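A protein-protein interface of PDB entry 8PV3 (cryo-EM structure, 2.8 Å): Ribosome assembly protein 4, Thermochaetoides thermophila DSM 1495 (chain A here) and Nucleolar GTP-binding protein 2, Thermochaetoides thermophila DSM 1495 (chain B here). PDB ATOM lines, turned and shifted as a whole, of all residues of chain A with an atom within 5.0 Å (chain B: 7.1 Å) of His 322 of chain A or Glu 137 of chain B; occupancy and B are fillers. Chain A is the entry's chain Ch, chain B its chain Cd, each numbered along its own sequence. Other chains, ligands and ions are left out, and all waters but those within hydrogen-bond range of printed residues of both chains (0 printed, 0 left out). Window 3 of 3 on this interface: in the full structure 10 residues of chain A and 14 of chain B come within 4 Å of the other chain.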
ATOM      1  N   SER A 298      18.710  19.530  13.098  1.00  0.00           N
ATOM      2  CA  SER A 298      18.199  18.199  12.806  1.00  0.00           C
ATOM      3  C   SER A 298      17.562  17.575  14.037  1.00  0.00           C
ATOM      4  O   SER A 298      17.598  18.127  15.138  1.00  0.00           O
ATOM      5  CB  SER A 298      19.294  17.289  12.263  1.00  0.00           C
ATOM      6  OG  SER A 298      18.821  15.963  12.120  1.00  0.00           O
ATOM      7  N   ARG A 301      19.253  16.260  17.706  1.00  0.00           N
ATOM      8  CA  ARG A 301      19.467  17.267  18.743  1.00  0.00           C
ATOM      9  C   ARG A 301      20.663  18.158  18.442  1.00  0.00           C
ATOM     10  O   ARG A 301      21.281  18.669  19.384  1.00  0.00           O
ATOM     11  CB  ARG A 301      19.642  16.636  20.129  1.00  0.00           C
ATOM     12  CG  ARG A 301      18.554  15.645  20.495  1.00  0.00           C
ATOM     13  CD  ARG A 301      18.852  14.954  21.805  1.00  0.00           C
ATOM     14  NE  ARG A 301      20.150  14.294  21.779  1.00  0.00           N
ATOM     15  CZ  ARG A 301      20.355  13.066  21.323  1.00  0.00           C
ATOM     16  NH1 ARG A 301      19.363  12.330  20.849  1.00  0.00           N
ATOM     17  NH2 ARG A 301      21.585  12.564  21.341  1.00  0.00           N
ATOM     18  N   HIS A 320      21.106  21.220  22.548  1.00  0.00           N
ATOM     19  CA  HIS A 320      19.677  20.957  22.661  1.00  0.00           C
ATOM     20  C   HIS A 320      19.426  19.554  23.195  1.00  0.00           C
ATOM     21  O   HIS A 320      20.234  18.643  23.001  1.00  0.00           O
ATOM     22  CB  HIS A 320      18.985  21.125  21.309  1.00  0.00           C
ATOM     23  CG  HIS A 320      18.757  22.551  20.910  1.00  0.00           C
ATOM     24  ND1 HIS A 320      17.896  23.384  21.590  1.00  0.00           N
ATOM     25  CD2 HIS A 320      19.263  23.284  19.892  1.00  0.00           C
ATOM     26  CE1 HIS A 320      17.881  24.569  21.007  1.00  0.00           C
ATOM     27  NE2 HIS A 320      18.709  24.537  19.980  1.00  0.00           N
ATOM     28  N   GLY A 321      18.297  19.384  23.875  1.00  0.00           N
ATOM     29  CA  GLY A 321      17.930  18.124  24.478  1.00  0.00           C
ATOM     30  C   GLY A 321      16.927  17.287  23.716  1.00  0.00           C
ATOM     31  O   GLY A 321      16.636  16.167  24.145  1.00  0.00           O
ATOM     32  N   HIS A 322      16.392  17.782  22.605  1.00  0.00           N
ATOM     33  CA  HIS A 322      15.422  17.033  21.816  1.00  0.00           C
ATOM     34  C   HIS A 322      15.527  17.513  20.371  1.00  0.00           C
ATOM     35  O   HIS A 322      16.513  18.150  19.987  1.00  0.00           O
ATOM     36  CB  HIS A 322      14.013  17.191  22.395  1.00  0.00           C
ATOM     37  CG  HIS A 322      13.143  15.985  22.213  1.00  0.00           C
ATOM     38  ND1 HIS A 322      12.389  15.769  21.081  1.00  0.00           N
ATOM     39  CD2 HIS A 322      12.899  14.935  23.032  1.00  0.00           C
ATOM     40  CE1 HIS A 322      11.725  14.634  21.205  1.00  0.00           C
ATOM     41  NE2 HIS A 322      12.016  14.109  22.380  1.00  0.00           N
ATOM     42  N   TRP A 323      14.516  17.181  19.562  1.00  0.00           N
ATOM     43  CA  TRP A 323      14.474  17.552  18.153  1.00  0.00           C
ATOM     44  C   TRP A 323      14.564  19.060  17.976  1.00  0.00           C
ATOM     45  O   TRP A 323      13.925  19.825  18.699  1.00  0.00           O
ATOM     46  CB  TRP A 323      13.170  17.082  17.511  1.00  0.00           C
ATOM     47  CG  TRP A 323      12.995  15.619  17.357  1.00  0.00           C
ATOM     48  CD1 TRP A 323      13.873  14.638  17.701  1.00  0.00           C
ATOM     49  CD2 TRP A 323      11.852  14.962  16.808  1.00  0.00           C
ATOM     50  NE1 TRP A 323      13.346  13.407  17.398  1.00  0.00           N
ATOM     51  CE2 TRP A 323      12.104  13.581  16.848  1.00  0.00           C
ATOM     52  CE3 TRP A 323      10.636  15.412  16.285  1.00  0.00           C
ATOM     53  CZ2 TRP A 323      11.186  12.645  16.384  1.00  0.00           C
ATOM     54  CZ3 TRP A 323       9.729  14.484  15.827  1.00  0.00           C
ATOM     55  CH2 TRP A 323      10.008  13.116  15.879  1.00  0.00           C
ATOM     56  N   VAL A 324      15.345  19.488  16.993  1.00  0.00           N
ATOM     57  CA  VAL A 324      15.410  20.896  16.623  1.00  0.00           C
ATOM     58  C   VAL A 324      14.440  21.136  15.475  1.00  0.00           C
ATOM     59  O   VAL A 324      14.569  20.536  14.402  1.00  0.00           O
ATOM     60  CB  VAL A 324      16.841  21.300  16.235  1.00  0.00           C
ATOM     61  CG1 VAL A 324      16.871  22.732  15.749  1.00  0.00           C
ATOM     62  CG2 VAL A 324      17.770  21.122  17.414  1.00  0.00           C
ATOM     63  N   SER A 379      13.767  24.203  20.082  1.00  0.00           N
ATOM     64  CA  SER A 379      13.702  22.749  20.116  1.00  0.00           C
ATOM     65  C   SER A 379      12.487  22.262  20.891  1.00  0.00           C
ATOM     66  O   SER A 379      11.759  23.040  21.511  1.00  0.00           O
ATOM     67  CB  SER A 379      14.975  22.148  20.711  1.00  0.00           C
ATOM     68  OG  SER A 379      15.391  22.879  21.846  1.00  0.00           O
ATOM     69  N   ASP A 380      12.276  20.943  20.831  1.00  0.00           N
ATOM     70  CA  ASP A 380      11.251  20.201  21.565  1.00  0.00           C
ATOM     71  C   ASP A 380      11.553  20.063  23.003  1.00  0.00           C
ATOM     72  O   ASP A 380      10.673  19.597  23.733  1.00  0.00           O
ATOM     73  CB  ASP A 380      11.057  18.808  20.970  1.00  0.00           C
ATOM     74  CG  ASP A 380      10.304  18.830  19.675  1.00  0.00           C
ATOM     75  OD1 ASP A 380       9.592  17.848  19.382  1.00  0.00           O
ATOM     76  OD2 ASP A 380      10.409  19.840  18.958  1.00  0.00           O
ATOM     77  N   ASP A 381      12.740  20.429  23.478  1.00  0.00           N
ATOM     78  CA  ASP A 381      13.048  20.367  24.898  1.00  0.00           C
ATOM     79  C   ASP A 381      12.542  21.581  25.661  1.00  0.00           C
ATOM     80  O   ASP A 381      13.066  21.877  26.739  1.00  0.00           O
ATOM     81  CB  ASP A 381      14.554  20.179  25.118  1.00  0.00           C
ATOM     82  CG  ASP A 381      15.399  21.270  24.482  1.00  0.00           C
ATOM     83  OD1 ASP A 381      14.858  22.272  23.975  1.00  0.00           O
ATOM     84  OD2 ASP A 381      16.639  21.131  24.502  1.00  0.00           O
ATOM     85  N   HIS B 130       8.101  17.539  32.704  1.00  0.00           N
ATOM     86  CA  HIS B 130       8.330  16.805  31.469  1.00  0.00           C
ATOM     87  C   HIS B 130       9.759  16.316  31.298  1.00  0.00           C
ATOM     88  O   HIS B 130      10.047  15.674  30.281  1.00  0.00           O
ATOM     89  CB  HIS B 130       7.959  17.666  30.256  1.00  0.00           C
ATOM     90  CG  HIS B 130       6.513  18.040  30.194  1.00  0.00           C
ATOM     91  ND1 HIS B 130       5.572  17.263  29.557  1.00  0.00           N
ATOM     92  CD2 HIS B 130       5.846  19.109  30.689  1.00  0.00           C
ATOM     93  CE1 HIS B 130       4.388  17.837  29.658  1.00  0.00           C
ATOM     94  NE2 HIS B 130       4.527  18.960  30.340  1.00  0.00           N
ATOM     95  N   GLN B 131      10.659  16.610  32.246  1.00  0.00           N
ATOM     96  CA  GLN B 131      12.055  16.189  32.121  1.00  0.00           C
ATOM     97  C   GLN B 131      12.204  14.672  32.030  1.00  0.00           C
ATOM     98  O   GLN B 131      13.016  14.173  31.243  1.00  0.00           O
ATOM     99  CB  GLN B 131      12.863  16.726  33.302  1.00  0.00           C
ATOM    100  CG  GLN B 131      14.365  16.682  33.101  1.00  0.00           C
ATOM    101  CD  GLN B 131      14.868  17.767  32.172  1.00  0.00           C
ATOM    102  OE1 GLN B 131      14.155  18.724  31.870  1.00  0.00           O
ATOM    103  NE2 GLN B 131      16.103  17.621  31.709  1.00  0.00           N
ATOM    104  N   ALA B 132      11.433  13.923  32.821  1.00  0.00           N
ATOM    105  CA  ALA B 132      11.563  12.467  32.831  1.00  0.00           C
ATOM    106  C   ALA B 132      11.141  11.858  31.498  1.00  0.00           C
ATOM    107  O   ALA B 132      11.877  11.058  30.904  1.00  0.00           O
ATOM    108  CB  ALA B 132      10.736  11.882  33.973  1.00  0.00           C
ATOM    109  N   LYS B 133       9.960  12.244  31.006  1.00  0.00           N
ATOM    110  CA  LYS B 133       9.484  11.757  29.714  1.00  0.00           C
ATOM    111  C   LYS B 133      10.395  12.216  28.582  1.00  0.00           C
ATOM    112  O   LYS B 133      10.603  11.486  27.607  1.00  0.00           O
ATOM    113  CB  LYS B 133       8.051  12.236  29.479  1.00  0.00           C
ATOM    114  CG  LYS B 133       7.414  11.717  28.203  1.00  0.00           C
ATOM    115  CD  LYS B 133       5.986  12.207  28.063  1.00  0.00           C
ATOM    116  CE  LYS B 133       5.947  13.679  27.694  1.00  0.00           C
ATOM    117  NZ  LYS B 133       4.561  14.159  27.451  1.00  0.00           N
ATOM    118  N   MET B 134      10.969  13.414  28.714  1.00  0.00           N
ATOM    119  CA  MET B 134      11.883  13.936  27.706  1.00  0.00           C
ATOM    120  C   MET B 134      13.159  13.109  27.637  1.00  0.00           C
ATOM    121  O   MET B 134      13.637  12.782  26.542  1.00  0.00           O
ATOM    122  CB  MET B 134      12.191  15.389  28.046  1.00  0.00           C
ATOM    123  CG  MET B 134      13.018  16.162  27.059  1.00  0.00           C
ATOM    124  SD  MET B 134      13.185  17.813  27.751  1.00  0.00           S
ATOM    125  CE  MET B 134      11.513  18.418  27.526  1.00  0.00           C
ATOM    126  N   THR B 135      13.714  12.747  28.798  1.00  0.00           N
ATOM    127  CA  THR B 135      14.912  11.913  28.821  1.00  0.00           C
ATOM    128  C   THR B 135      14.625  10.515  28.295  1.00  0.00           C
ATOM    129  O   THR B 135      15.468   9.922  27.615  1.00  0.00           O
ATOM    130  CB  THR B 135      15.487  11.830  30.236  1.00  0.00           C
ATOM    131  OG1 THR B 135      14.467  11.418  31.151  1.00  0.00           O
ATOM    132  CG2 THR B 135      16.059  13.173  30.668  1.00  0.00           C
ATOM    133  N   ILE B 136      13.445   9.969  28.601  1.00  0.00           N
ATOM    134  CA  ILE B 136      13.110   8.640  28.088  1.00  0.00           C
ATOM    135  C   ILE B 136      12.912   8.670  26.572  1.00  0.00           C
ATOM    136  O   ILE B 136      13.320   7.737  25.869  1.00  0.00           O
ATOM    137  CB  ILE B 136      11.880   8.074  28.824  1.00  0.00           C
ATOM    138  CG1 ILE B 136      12.182   7.926  30.312  1.00  0.00           C
ATOM    139  CG2 ILE B 136      11.483   6.719  28.275  1.00  0.00           C
ATOM    140  CD1 ILE B 136      13.441   7.142  30.606  1.00  0.00           C
ATOM    141  N   GLU B 137      12.312   9.739  26.040  1.00  0.00           N
ATOM    142  CA  GLU B 137      12.181   9.869  24.591  1.00  0.00           C
ATOM    143  C   GLU B 137      13.537  10.043  23.919  1.00  0.00           C
ATOM    144  O   GLU B 137      13.760   9.520  22.821  1.00  0.00           O
ATOM    145  CB  GLU B 137      11.263  11.040  24.244  1.00  0.00           C
ATOM    146  CG  GLU B 137       9.790  10.756  24.458  1.00  0.00           C
ATOM    147  CD  GLU B 137       8.933  11.997  24.320  1.00  0.00           C
ATOM    148  OE1 GLU B 137       9.496  13.112  24.341  1.00  0.00           O
ATOM    149  OE2 GLU B 137       7.699  11.860  24.188  1.00  0.00           O
ATOM    150  N   ARG B 138      14.448  10.790  24.549  1.00  0.00           N
ATOM    151  CA  ARG B 138      15.785  10.955  23.988  1.00  0.00           C
ATOM    152  C   ARG B 138      16.569   9.648  24.008  1.00  0.00           C
ATOM    153  O   ARG B 138      17.198   9.280  23.010  1.00  0.00           O
ATOM    154  CB  ARG B 138      16.545  12.034  24.754  1.00  0.00           C
ATOM    155  CG  ARG B 138      17.939  12.301  24.226  1.00  0.00           C
ATOM    156  CD  ARG B 138      18.787  13.104  25.206  1.00  0.00           C
ATOM    157  NE  ARG B 138      18.036  14.169  25.860  1.00  0.00           N
ATOM    158  CZ  ARG B 138      17.757  14.200  27.156  1.00  0.00           C
ATOM    159  NH1 ARG B 138      18.168  13.245  27.972  1.00  0.00           N
ATOM    160  NH2 ARG B 138      17.050  15.214  27.643  1.00  0.00           N
ATOM    161  N   GLU B 139      16.541   8.934  25.130  1.00  0.00           N
ATOM    162  CA  GLU B 139      17.309   7.706  25.318  1.00  0.00           C
ATOM    163  C   GLU B 139      16.385   6.664  25.935  1.00  0.00           C
ATOM    164  O   GLU B 139      16.058   6.758  27.131  1.00  0.00           O
ATOM    165  CB  GLU B 139      18.519   7.951  26.210  1.00  0.00           C
ATOM    166  CG  GLU B 139      19.551   8.900  25.621  1.00  0.00           C
ATOM    167  CD  GLU B 139      20.669   9.226  26.590  1.00  0.00           C
ATOM    168  OE1 GLU B 139      20.578   8.816  27.765  1.00  0.00           O
ATOM    169  OE2 GLU B 139      21.634   9.903  26.178  1.00  0.00           O
ATOM    170  N   PRO B 140      15.937   5.674  25.164  1.00  0.00           N
ATOM    171  CA  PRO B 140      15.012   4.675  25.715  1.00  0.00           C
ATOM    172  C   PRO B 140      15.697   3.753  26.712  1.00  0.00           C
ATOM    173  O   PRO B 140      16.921   3.745  26.850  1.00  0.00           O
ATOM    174  CB  PRO B 140      14.538   3.900  24.479  1.00  0.00           C
ATOM    175  CG  PRO B 140      15.473   4.253  23.394  1.00  0.00           C
ATOM    176  CD  PRO B 140      16.054   5.584  23.701  1.00  0.00           C
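A ring nitrogen (NE2) of His 322 of chain A lies within hydrogen-bond range of the side-chain carboxylate of Glu 137 of chain B. O of Gly 321 of chain A is in hydrogen-bond range of NE of Arg 138 of chain B, at 3.0 Å.
The side-chain carboxylate of Asp 381 of chain A is in hydrogen-bond range of the backbone NH of Gly 321 of chain A (2.5 Å). The side-chain hydroxyl (OG) of Ser 379 of chain A sits close to the side-chain carboxylate (OD2) of Asp 381 of chain A.
Among the printed residues, merely in contact across the chains: Asp 381 of chain A with Met 134 of chain B and Arg 301 of chain A with Arg 138 of chain B.
Ser 298 of chain A touches none of the printed residues of chain B. Printed residues of chain B within 4 Å of Arg 301 of chain A: Arg 138 (3.7 Å). Gly 321 of chain A touches just one residue of chain B: Arg 138 (3.0 Å). Of the printed residues of chain B, His 322 of chain A touches Glu 137 (3.3 Å). Of the printed residues of chain A, Met 134 of chain B touches Asp 381 (3.6 Å). Glu 137 of chain B touches just one residue of chain A: His 322 (3.3 Å). Of the printed residues of chain A, Arg 138 of chain B touches Arg 301 and Gly 321. The nearest residue of chain B that does not touch His 322 of chain A is Met 134 of chain B (4.2 Å). The nearest printed residue of chain A that does not touch Glu 137 of chain B is Arg 301 of chain A (6.6 Å).
Printed residues of chain A that touch a printed residue of chain B: Arg 301, Gly 321, His 322 and Asp 381. Hydrophobic or aromatic side chains of chain A that line the printed part of chain B: His 322. Among the printed residues, 4 pairs touch across the chains. Among the printed residues, no Asp or Glu carboxylate lies within 4 Å of a Lys or Arg side-chain nitrogen of the other chain.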
